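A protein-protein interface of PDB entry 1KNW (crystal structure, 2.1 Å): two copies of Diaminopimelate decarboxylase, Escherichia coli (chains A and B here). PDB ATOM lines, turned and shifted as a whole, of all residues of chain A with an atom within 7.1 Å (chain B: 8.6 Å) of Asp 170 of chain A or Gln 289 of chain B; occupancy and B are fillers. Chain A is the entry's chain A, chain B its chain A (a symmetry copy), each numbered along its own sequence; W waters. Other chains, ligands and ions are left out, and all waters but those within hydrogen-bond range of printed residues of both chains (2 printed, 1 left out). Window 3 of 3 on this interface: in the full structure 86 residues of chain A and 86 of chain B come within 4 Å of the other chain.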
ATOM      1  N   VAL A 124      -4.859  -8.638 -10.156  1.00  0.00           N
ATOM      2  CA  VAL A 124      -3.480  -9.122  -9.975  1.00  0.00           C
ATOM      3  C   VAL A 124      -3.070  -9.011  -8.505  1.00  0.00           C
ATOM      4  O   VAL A 124      -2.394  -9.893  -7.974  1.00  0.00           O
ATOM      5  CB  VAL A 124      -2.494  -8.328 -10.850  1.00  0.00           C
ATOM      6  CG1 VAL A 124      -1.043  -8.610 -10.460  1.00  0.00           C
ATOM      7  CG2 VAL A 124      -2.697  -8.650 -12.327  1.00  0.00           C
ATOM      8  N   GLU A 160     -14.002  -1.129 -19.640  1.00  0.00           N
ATOM      9  CA  GLU A 160     -13.346  -0.227 -18.716  1.00  0.00           C
ATOM     10  C   GLU A 160     -14.224   0.326 -17.631  1.00  0.00           C
ATOM     11  O   GLU A 160     -13.696   0.781 -16.593  1.00  0.00           O
ATOM     12  CB  GLU A 160     -12.641   0.912 -19.486  1.00  0.00           C
ATOM     13  CG  GLU A 160     -13.611   1.867 -20.145  1.00  0.00           C
ATOM     14  CD  GLU A 160     -12.927   2.963 -20.943  1.00  0.00           C
ATOM     15  OE1 GLU A 160     -13.667   3.778 -21.542  1.00  0.00           O
ATOM     16  OE2 GLU A 160     -11.688   3.027 -20.953  1.00  0.00           O
ATOM     17  N   GLY A 165     -12.462  -8.506 -13.031  1.00  0.00           N
ATOM     18  CA  GLY A 165     -11.481  -9.245 -13.739  1.00  0.00           C
ATOM     19  C   GLY A 165     -10.208  -8.507 -14.100  1.00  0.00           C
ATOM     20  O   GLY A 165     -10.039  -7.326 -13.818  1.00  0.00           O
ATOM     21  N   ILE A 166      -9.193  -9.303 -14.446  1.00  0.00           N
ATOM     22  CA  ILE A 166      -7.893  -8.734 -14.832  1.00  0.00           C
ATOM     23  C   ILE A 166      -8.000  -8.168 -16.242  1.00  0.00           C
ATOM     24  O   ILE A 166      -8.355  -8.896 -17.178  1.00  0.00           O
ATOM     25  CB  ILE A 166      -6.805  -9.820 -14.768  1.00  0.00           C
ATOM     26  CG1 ILE A 166      -6.657 -10.325 -13.316  1.00  0.00           C
ATOM     27  CG2 ILE A 166      -5.469  -9.312 -15.286  1.00  0.00           C
ATOM     28  CD1 ILE A 166      -5.956 -11.693 -13.260  1.00  0.00           C
ATOM     29  N   TRP A 167      -7.738  -6.879 -16.381  1.00  0.00           N
ATOM     30  CA  TRP A 167      -7.771  -6.254 -17.722  1.00  0.00           C
ATOM     31  C   TRP A 167      -6.850  -7.048 -18.633  1.00  0.00           C
ATOM     32  O   TRP A 167      -5.684  -7.307 -18.246  1.00  0.00           O
ATOM     33  CB  TRP A 167      -7.299  -4.801 -17.618  1.00  0.00           C
ATOM     34  CG  TRP A 167      -7.538  -3.999 -18.864  1.00  0.00           C
ATOM     35  CD1 TRP A 167      -6.593  -3.540 -19.731  1.00  0.00           C
ATOM     36  CD2 TRP A 167      -8.800  -3.572 -19.388  1.00  0.00           C
ATOM     37  NE1 TRP A 167      -7.184  -2.851 -20.761  1.00  0.00           N
ATOM     38  CE2 TRP A 167      -8.543  -2.868 -20.583  1.00  0.00           C
ATOM     39  CE3 TRP A 167     -10.125  -3.715 -18.967  1.00  0.00           C
ATOM     40  CZ2 TRP A 167      -9.555  -2.288 -21.341  1.00  0.00           C
ATOM     41  CZ3 TRP A 167     -11.124  -3.141 -19.716  1.00  0.00           C
ATOM     42  CH2 TRP A 167     -10.841  -2.436 -20.902  1.00  0.00           C
ATOM     43  N   TYR A 168      -7.271  -7.354 -19.837  1.00  0.00           N
ATOM     44  CA  TYR A 168      -6.522  -8.232 -20.730  1.00  0.00           C
ATOM     45  C   TYR A 168      -5.096  -7.819 -20.972  1.00  0.00           C
ATOM     46  O   TYR A 168      -4.195  -8.699 -20.986  1.00  0.00           O
ATOM     47  CB  TYR A 168      -7.286  -8.473 -22.027  1.00  0.00           C
ATOM     48  CG  TYR A 168      -7.363  -7.310 -22.985  1.00  0.00           C
ATOM     49  CD1 TYR A 168      -6.638  -7.333 -24.176  1.00  0.00           C
ATOM     50  CD2 TYR A 168      -8.152  -6.200 -22.726  1.00  0.00           C
ATOM     51  CE1 TYR A 168      -6.702  -6.279 -25.068  1.00  0.00           C
ATOM     52  CE2 TYR A 168      -8.216  -5.138 -23.611  1.00  0.00           C
ATOM     53  CZ  TYR A 168      -7.487  -5.189 -24.786  1.00  0.00           C
ATOM     54  OH  TYR A 168      -7.539  -4.139 -25.677  1.00  0.00           O
ATOM     55  N   THR A 169      -4.764  -6.527 -20.968  1.00  0.00           N
ATOM     56  CA  THR A 169      -3.383  -6.102 -21.153  1.00  0.00           C
ATOM     57  C   THR A 169      -2.574  -6.168 -19.864  1.00  0.00           C
ATOM     58  O   THR A 169      -1.358  -5.930 -19.890  1.00  0.00           O
ATOM     59  CB  THR A 169      -3.248  -4.708 -21.776  1.00  0.00           C
ATOM     60  OG1 THR A 169      -3.620  -3.706 -20.823  1.00  0.00           O
ATOM     61  CG2 THR A 169      -4.117  -4.586 -23.018  1.00  0.00           C
ATOM     62  N   ASP A 170      -3.204  -6.558 -18.760  1.00  0.00           N
ATOM     63  CA  ASP A 170      -2.511  -6.802 -17.508  1.00  0.00           C
ATOM     64  C   ASP A 170      -2.119  -8.269 -17.343  1.00  0.00           C
ATOM     65  O   ASP A 170      -1.482  -8.632 -16.352  1.00  0.00           O
ATOM     66  CB  ASP A 170      -3.357  -6.368 -16.310  1.00  0.00           C
ATOM     67  CG  ASP A 170      -3.299  -4.889 -16.019  1.00  0.00           C
ATOM     68  OD1 ASP A 170      -2.379  -4.203 -16.501  1.00  0.00           O
ATOM     69  OD2 ASP A 170      -4.193  -4.387 -15.292  1.00  0.00           O
ATOM     70  N   LEU A 171      -2.415  -9.102 -18.347  1.00  0.00           N
ATOM     71  CA  LEU A 171      -2.089 -10.507 -18.321  1.00  0.00           C
ATOM     72  C   LEU A 171      -0.644 -10.845 -18.133  1.00  0.00           C
ATOM     73  O   LEU A 171      -0.296 -11.687 -17.275  1.00  0.00           O
ATOM     74  CB  LEU A 171      -2.733 -11.258 -19.498  1.00  0.00           C
ATOM     75  CG  LEU A 171      -4.237 -11.567 -19.290  1.00  0.00           C
ATOM     76  CD1 LEU A 171      -4.875 -12.117 -20.544  1.00  0.00           C
ATOM     77  CD2 LEU A 171      -4.412 -12.535 -18.124  1.00  0.00           C
ATOM     78  N   PRO A 172       0.280 -10.177 -18.810  1.00  0.00           N
ATOM     79  CA  PRO A 172       1.710 -10.385 -18.606  1.00  0.00           C
ATOM     80  C   PRO A 172       2.108 -10.129 -17.164  1.00  0.00           C
ATOM     81  O   PRO A 172       2.848 -10.926 -16.573  1.00  0.00           O
ATOM     82  CB  PRO A 172       2.378  -9.409 -19.562  1.00  0.00           C
ATOM     83  CG  PRO A 172       1.345  -9.166 -20.620  1.00  0.00           C
ATOM     84  CD  PRO A 172       0.013  -9.203 -19.888  1.00  0.00           C
ATOM     85  N   ALA A 173       1.527  -9.102 -16.537  1.00  0.00           N
ATOM     86  CA  ALA A 173       1.785  -8.830 -15.124  1.00  0.00           C
ATOM     87  C   ALA A 173       1.218  -9.927 -14.232  1.00  0.00           C
ATOM     88  O   ALA A 173       1.827 -10.302 -13.228  1.00  0.00           O
ATOM     89  CB  ALA A 173       1.209  -7.473 -14.731  1.00  0.00           C
ATOM     90  N   ALA A 174       0.083 -10.507 -14.626  1.00  0.00           N
ATOM     91  CA  ALA A 174      -0.487 -11.638 -13.884  1.00  0.00           C
ATOM     92  C   ALA A 174       0.425 -12.854 -13.983  1.00  0.00           C
ATOM     93  O   ALA A 174       0.624 -13.563 -12.994  1.00  0.00           O
ATOM     94  CB  ALA A 174      -1.879 -11.962 -14.376  1.00  0.00           C
ATOM     95  N   LEU A 175       1.017 -13.085 -15.153  1.00  0.00           N
ATOM     96  CA  LEU A 175       1.929 -14.212 -15.327  1.00  0.00           C
ATOM     97  C   LEU A 175       3.151 -14.083 -14.428  1.00  0.00           C
ATOM     98  O   LEU A 175       3.558 -15.047 -13.784  1.00  0.00           O
ATOM     99  CB  LEU A 175       2.366 -14.356 -16.791  1.00  0.00           C
ATOM    100  CG  LEU A 175       3.369 -15.478 -17.080  1.00  0.00           C
ATOM    101  CD1 LEU A 175       2.809 -16.821 -16.588  1.00  0.00           C
ATOM    102  CD2 LEU A 175       3.682 -15.565 -18.572  1.00  0.00           C
ATOM    103  N   ASP A 176       3.696 -12.871 -14.303  1.00  0.00           N
ATOM    104  CA  ASP A 176       4.822 -12.648 -13.389  1.00  0.00           C
ATOM    105  C   ASP A 176       4.446 -13.068 -11.968  1.00  0.00           C
ATOM    106  O   ASP A 176       5.267 -13.640 -11.242  1.00  0.00           O
ATOM    107  CB  ASP A 176       5.285 -11.213 -13.428  1.00  0.00           C
ATOM    108  CG  ASP A 176       5.947 -10.780 -14.713  1.00  0.00           C
ATOM    109  OD1 ASP A 176       6.480 -11.627 -15.461  1.00  0.00           O
ATOM    110  OD2 ASP A 176       5.939  -9.552 -14.992  1.00  0.00           O
ATOM    111  N   PHE A 215      -1.944 -15.664 -24.199  1.00  0.00           N
ATOM    112  CA  PHE A 215      -1.327 -15.819 -22.878  1.00  0.00           C
ATOM    113  C   PHE A 215      -0.261 -16.914 -22.898  1.00  0.00           C
ATOM    114  O   PHE A 215       0.731 -16.844 -22.175  1.00  0.00           O
ATOM    115  CB  PHE A 215      -2.379 -16.110 -21.822  1.00  0.00           C
ATOM    116  CG  PHE A 215      -1.935 -15.924 -20.398  1.00  0.00           C
ATOM    117  CD1 PHE A 215      -1.233 -14.800 -20.006  1.00  0.00           C
ATOM    118  CD2 PHE A 215      -2.246 -16.881 -19.440  1.00  0.00           C
ATOM    119  CE1 PHE A 215      -0.837 -14.631 -18.689  1.00  0.00           C
ATOM    120  CE2 PHE A 215      -1.851 -16.717 -18.126  1.00  0.00           C
ATOM    121  CZ  PHE A 215      -1.149 -15.595 -17.744  1.00  0.00           C
ATOM    122  N   SER B 286      -7.812  -4.155  -3.566  1.00  0.00           N
ATOM    123  CA  SER B 286      -7.260  -4.288  -4.899  1.00  0.00           C
ATOM    124  C   SER B 286      -7.248  -2.922  -5.608  1.00  0.00           C
ATOM    125  O   SER B 286      -8.207  -2.160  -5.506  1.00  0.00           O
ATOM    126  CB  SER B 286      -8.057  -5.261  -5.769  1.00  0.00           C
ATOM    127  OG  SER B 286      -8.007  -6.591  -5.308  1.00  0.00           O
ATOM    128  N   VAL B 287      -6.130  -2.629  -6.237  1.00  0.00           N
ATOM    129  CA  VAL B 287      -5.964  -1.416  -7.025  1.00  0.00           C
ATOM    130  C   VAL B 287      -5.485  -1.841  -8.428  1.00  0.00           C
ATOM    131  O   VAL B 287      -4.522  -2.612  -8.530  1.00  0.00           O
ATOM    132  CB  VAL B 287      -4.926  -0.461  -6.426  1.00  0.00           C
ATOM    133  CG1 VAL B 287      -4.839   0.817  -7.280  1.00  0.00           C
ATOM    134  CG2 VAL B 287      -5.260  -0.091  -4.987  1.00  0.00           C
ATOM    135  N   LYS B 288      -6.223  -1.438  -9.451  1.00  0.00           N
ATOM    136  CA  LYS B 288      -5.876  -1.849 -10.807  1.00  0.00           C
ATOM    137  C   LYS B 288      -6.361  -0.855 -11.850  1.00  0.00           C
ATOM    138  O   LYS B 288      -7.321  -0.107 -11.626  1.00  0.00           O
ATOM    139  CB  LYS B 288      -6.467  -3.237 -11.110  1.00  0.00           C
ATOM    140  CG  LYS B 288      -7.995  -3.239 -11.129  1.00  0.00           C
ATOM    141  CD  LYS B 288      -8.540  -4.663 -11.249  1.00  0.00           C
ATOM    142  CE  LYS B 288     -10.058  -4.664 -11.001  1.00  0.00           C
ATOM    143  NZ  LYS B 288     -10.626  -6.037 -11.166  1.00  0.00           N
ATOM    144  N   GLN B 289      -5.714  -0.897 -13.011  1.00  0.00           N
ATOM    145  CA  GLN B 289      -6.123  -0.058 -14.141  1.00  0.00           C
ATOM    146  C   GLN B 289      -7.023  -0.885 -15.063  1.00  0.00           C
ATOM    147  O   GLN B 289      -6.659  -2.019 -15.412  1.00  0.00           O
ATOM    148  CB  GLN B 289      -4.880   0.395 -14.912  1.00  0.00           C
ATOM    149  CG  GLN B 289      -5.070   1.547 -15.858  1.00  0.00           C
ATOM    150  CD  GLN B 289      -5.394   2.857 -15.159  1.00  0.00           C
ATOM    151  OE1 GLN B 289      -6.019   3.744 -15.752  1.00  0.00           O
ATOM    152  NE2 GLN B 289      -4.987   2.981 -13.910  1.00  0.00           N
ATOM    153  N   MET B 290      -8.205  -0.386 -15.362  1.00  0.00           N
ATOM    154  CA  MET B 290      -9.077  -1.017 -16.358  1.00  0.00           C
ATOM    155  C   MET B 290      -9.216  -0.068 -17.556  1.00  0.00           C
ATOM    156  O   MET B 290      -9.976   0.893 -17.500  1.00  0.00           O
ATOM    157  CB  MET B 290     -10.463  -1.316 -15.777  1.00  0.00           C
ATOM    158  CG  MET B 290     -10.401  -1.972 -14.390  1.00  0.00           C
ATOM    159  SD  MET B 290      -9.694  -3.653 -14.516  1.00  0.00           S
ATOM    160  CE  MET B 290     -11.199  -4.530 -15.003  1.00  0.00           C
ATOM    161  N   GLY B 291      -8.424  -0.322 -18.593  1.00  0.00           N
ATOM    162  CA  GLY B 291      -8.448   0.579 -19.770  1.00  0.00           C
ATOM    163  C   GLY B 291      -8.011   1.976 -19.300  1.00  0.00           C
ATOM    164  O   GLY B 291      -7.014   2.086 -18.593  1.00  0.00           O
ATOM    165  N   SER B 292      -8.903   2.954 -19.447  1.00  0.00           N
ATOM    166  CA  SER B 292      -8.612   4.310 -19.016  1.00  0.00           C
ATOM    167  C   SER B 292      -9.078   4.600 -17.601  1.00  0.00           C
ATOM    168  O   SER B 292      -8.920   5.739 -17.125  1.00  0.00           O
ATOM    169  CB  SER B 292      -9.275   5.328 -19.971  1.00  0.00           C
ATOM    170  OG  SER B 292     -10.680   5.320 -19.772  1.00  0.00           O
ATOM    171  N   ARG B 293      -9.626   3.608 -16.904  1.00  0.00           N
ATOM    172  CA  ARG B 293     -10.099   3.817 -15.545  1.00  0.00           C
ATOM    173  C   ARG B 293      -9.123   3.308 -14.493  1.00  0.00           C
ATOM    174  O   ARG B 293      -8.611   2.194 -14.562  1.00  0.00           O
ATOM    175  CB  ARG B 293     -11.472   3.159 -15.341  1.00  0.00           C
ATOM    176  CG  ARG B 293     -12.540   3.686 -16.297  1.00  0.00           C
ATOM    177  CD  ARG B 293     -12.868   5.144 -15.992  1.00  0.00           C
ATOM    178  NE  ARG B 293     -14.248   5.447 -16.399  1.00  0.00           N
ATOM    179  CZ  ARG B 293     -14.723   6.682 -16.521  1.00  0.00           C
ATOM    180  NH1 ARG B 293     -15.983   6.866 -16.878  1.00  0.00           N
ATOM    181  NH2 ARG B 293     -13.930   7.721 -16.271  1.00  0.00           N
ATOM    182  N   HIS B 294      -8.956   4.103 -13.437  1.00  0.00           N
ATOM    183  CA  HIS B 294      -8.175   3.683 -12.276  1.00  0.00           C
ATOM    184  C   HIS B 294      -9.129   3.225 -11.170  1.00  0.00           C
ATOM    185  O   HIS B 294      -9.857   4.039 -10.605  1.00  0.00           O
ATOM    186  CB  HIS B 294      -7.301   4.841 -11.788  1.00  0.00           C
ATOM    187  CG  HIS B 294      -6.350   4.439 -10.703  1.00  0.00           C
ATOM    188  ND1 HIS B 294      -6.494   4.873  -9.398  1.00  0.00           N
ATOM    189  CD2 HIS B 294      -5.293   3.598 -10.709  1.00  0.00           C
ATOM    190  CE1 HIS B 294      -5.552   4.335  -8.657  1.00  0.00           C
ATOM    191  NE2 HIS B 294      -4.795   3.569  -9.427  1.00  0.00           N
ATOM    192  N   PHE B 295      -9.146   1.931 -10.891  1.00  0.00           N
ATOM    193  CA  PHE B 295     -10.073   1.342  -9.949  1.00  0.00           C
ATOM    194  C   PHE B 295      -9.446   1.070  -8.586  1.00  0.00           C
ATOM    195  O   PHE B 295      -8.359   0.518  -8.484  1.00  0.00           O
ATOM    196  CB  PHE B 295     -10.614   0.005 -10.501  1.00  0.00           C
ATOM    197  CG  PHE B 295     -11.886   0.142 -11.288  1.00  0.00           C
ATOM    198  CD1 PHE B 295     -11.859   0.529 -12.616  1.00  0.00           C
ATOM    199  CD2 PHE B 295     -13.115  -0.087 -10.689  1.00  0.00           C
ATOM    200  CE1 PHE B 295     -13.029   0.653 -13.344  1.00  0.00           C
ATOM    201  CE2 PHE B 295     -14.287   0.019 -11.410  1.00  0.00           C
ATOM    202  CZ  PHE B 295     -14.245   0.387 -12.752  1.00  0.00           C
ATOM    203  N   VAL B 296     -10.190   1.384  -7.529  1.00  0.00           N
ATOM    204  CA  VAL B 296      -9.804   1.019  -6.169  1.00  0.00           C
ATOM    205  C   VAL B 296     -10.971   0.228  -5.538  1.00  0.00           C
ATOM    206  O   VAL B 296     -12.078   0.751  -5.487  1.00  0.00           O
ATOM    207  CB  VAL B 296      -9.501   2.248  -5.312  1.00  0.00           C
ATOM    208  CG1 VAL B 296      -9.409   1.883  -3.831  1.00  0.00           C
ATOM    209  CG2 VAL B 296      -8.202   2.921  -5.767  1.00  0.00           C
ATOM    210  N   LEU B 297     -10.756  -1.052  -5.284  1.00  0.00           N
ATOM    211  CA  LEU B 297     -11.780  -1.912  -4.719  1.00  0.00           C
ATOM    212  C   LEU B 297     -11.564  -2.090  -3.200  1.00  0.00           C
ATOM    213  O   LEU B 297     -10.467  -2.437  -2.778  1.00  0.00           O
ATOM    214  CB  LEU B 297     -11.830  -3.284  -5.355  1.00  0.00           C
ATOM    215  CG  LEU B 297     -11.850  -3.507  -6.829  1.00  0.00           C
ATOM    216  CD1 LEU B 297     -12.694  -4.731  -7.220  1.00  0.00           C
ATOM    217  CD2 LEU B 297     -12.212  -2.323  -7.672  1.00  0.00           C
ATOM    218  N   VAL B 333      -5.658  11.376  -7.862  1.00  0.00           N
ATOM    219  CA  VAL B 333      -5.885  10.744  -9.148  1.00  0.00           C
ATOM    220  C   VAL B 333      -7.385  10.421  -9.292  1.00  0.00           C
ATOM    221  O   VAL B 333      -8.036  10.126  -8.287  1.00  0.00           O
ATOM    222  CB  VAL B 333      -5.076   9.468  -9.366  1.00  0.00           C
ATOM    223  CG1 VAL B 333      -3.567   9.747  -9.364  1.00  0.00           C
ATOM    224  CG2 VAL B 333      -5.402   8.406  -8.332  1.00  0.00           C
ATOM    225  N   GLU B 334      -7.924  10.641 -10.478  1.00  0.00           N
ATOM    226  CA  GLU B 334      -9.344  10.340 -10.717  1.00  0.00           C
ATOM    227  C   GLU B 334      -9.580   8.841 -10.539  1.00  0.00           C
ATOM    228  O   GLU B 334      -8.972   8.023 -11.232  1.00  0.00           O
ATOM    229  CB  GLU B 334      -9.774  10.823 -12.088  1.00  0.00           C
ATOM    230  CG  GLU B 334      -9.839  12.341 -12.238  1.00  0.00           C
ATOM    231  CD  GLU B 334     -10.756  12.987 -11.218  1.00  0.00           C
ATOM    232  OE1 GLU B 334     -11.777  12.362 -10.843  1.00  0.00           O
ATOM    233  OE2 GLU B 334     -10.432  14.098 -10.751  1.00  0.00           O
ATOM    234  N   THR B 335     -10.361   8.488  -9.528  1.00  0.00           N
ATOM    235  CA  THR B 335     -10.491   7.083  -9.121  1.00  0.00           C
ATOM    236  C   THR B 335     -11.928   6.594  -9.206  1.00  0.00           C
ATOM    237  O   THR B 335     -12.840   7.299  -8.758  1.00  0.00           O
ATOM    238  CB  THR B 335     -10.037   6.953  -7.634  1.00  0.00           C
ATOM    239  OG1 THR B 335      -8.709   7.452  -7.517  1.00  0.00           O
ATOM    240  CG2 THR B 335     -10.104   5.510  -7.181  1.00  0.00           C
ATOM    241  N   GLU B 363      -3.598   8.482  -4.118  1.00  0.00           N
ATOM    242  CA  GLU B 363      -3.317   7.191  -4.740  1.00  0.00           C
ATOM    243  C   GLU B 363      -3.036   6.112  -3.709  1.00  0.00           C
ATOM    244  O   GLU B 363      -1.882   5.749  -3.461  1.00  0.00           O
ATOM    245  CB  GLU B 363      -2.135   7.341  -5.702  1.00  0.00           C
ATOM    246  CG  GLU B 363      -1.859   6.106  -6.549  1.00  0.00           C
ATOM    247  CD  GLU B 363      -0.990   6.447  -7.753  1.00  0.00           C
ATOM    248  OE1 GLU B 363      -0.432   7.562  -7.786  1.00  0.00           O
ATOM    249  OE2 GLU B 363      -0.878   5.590  -8.653  1.00  0.00           O
HETATM  250  O   HOH W   1      -4.375  -2.050 -17.468  1.00  0.00           O
HETATM  251  O   HOH W   2      -3.633  -2.752 -13.470  1.00  0.00           O
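Of chain B, only Gln 289 comes within 4 Å of Asp 170 of chain A.
Printed residues of chain A within 4 Å of Ser 292 of chain B: Glu 160.
Of the printed residues of chain A, Lys 288 of chain B touches Gly 165.
Of the printed residues of chain A, Gly 291 of chain B touches Trp 167 (3.2 Å).
His 294 of chain B touches none of the printed residues of chain A.
Glu 363 of chain B touches none of the printed residues of chain A.
The nearest residue of chain B that does not touch Asp 170 of chain A is Lys 288 of chain B (4.9 Å).
The nearest printed residue of chain A that does not touch Ser 292 of chain B is Trp 167 of chain A (5.6 Å).
No position is printed for both chains.
O of Lys 288 of chain B sits at hydrogen-bond distance from N of Phe 295 of chain B, at 2.8 Å.
The side-chain amide oxygen (OE1) of Gln 289 of chain B lies close to the backbone carbonyl oxygen (O) of Gly 291 of chain B (3.4 Å).
The side-chain amide oxygen (OE1) of Gln 289 of chain B lies close to the backbone carbonyl oxygen (O) of Arg 293 of chain B (3.2 Å).
Water W2 bridges the side-chain carboxylate (OD2) of Asp 170 of chain A (2.5 Å) and the backbone NH (N) of Gln 289 of chain B (2.8 Å).
Water W1 lies within hydrogen-bond range of the backbone carbonyl oxygen (O) of Gln 289 of chain B and the side-chain carboxylate (OD1) of Asp 170 of chain A.
The side-chain hydroxyl (OG) of Ser 292 of chain B sits at hydrogen-bond distance from the side-chain carboxylate (OE2) of Glu 160 of chain A (2.8 Å).
The backbone carbonyl oxygen (O) of Gly 165 of chain A lies within hydrogen-bond range of the side-chain amino group (NZ) of Lys 288 of chain B (3.0 Å).
SD of Met 290 of chain B lies close to O of Gly 165 of chain A (3.8 Å).
The backbone carbonyl oxygen (O) of Gln 289 of chain B lies close to the side-chain carboxylate (OD2) of Asp 170 of chain A, 3.4 Å away.
Glu 160 of chain A touches Met 290 of chain B.
Glu 160 of chain A touches Arg 293 of chain B (O to CG, 3.1 Å).
CE1 of Phe 295 of chain B touches O of Glu 160 of chain A (3.3 Å).
Gln 289 of chain B touches Trp 167 of chain A (O to CB, 3.6 Å).
Trp 167 of chain A touches Met 290 of chain B.
Trp 167 of chain A touches Gly 291 of chain B.
Of the 16 printed residues of chain B, 7 touch a printed residue of chain A.
Hydrophobic or aromatic side chains of chain A that line the printed part of chain B: Trp 167.
Among the printed residues, 10 pairs touch across the chains.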
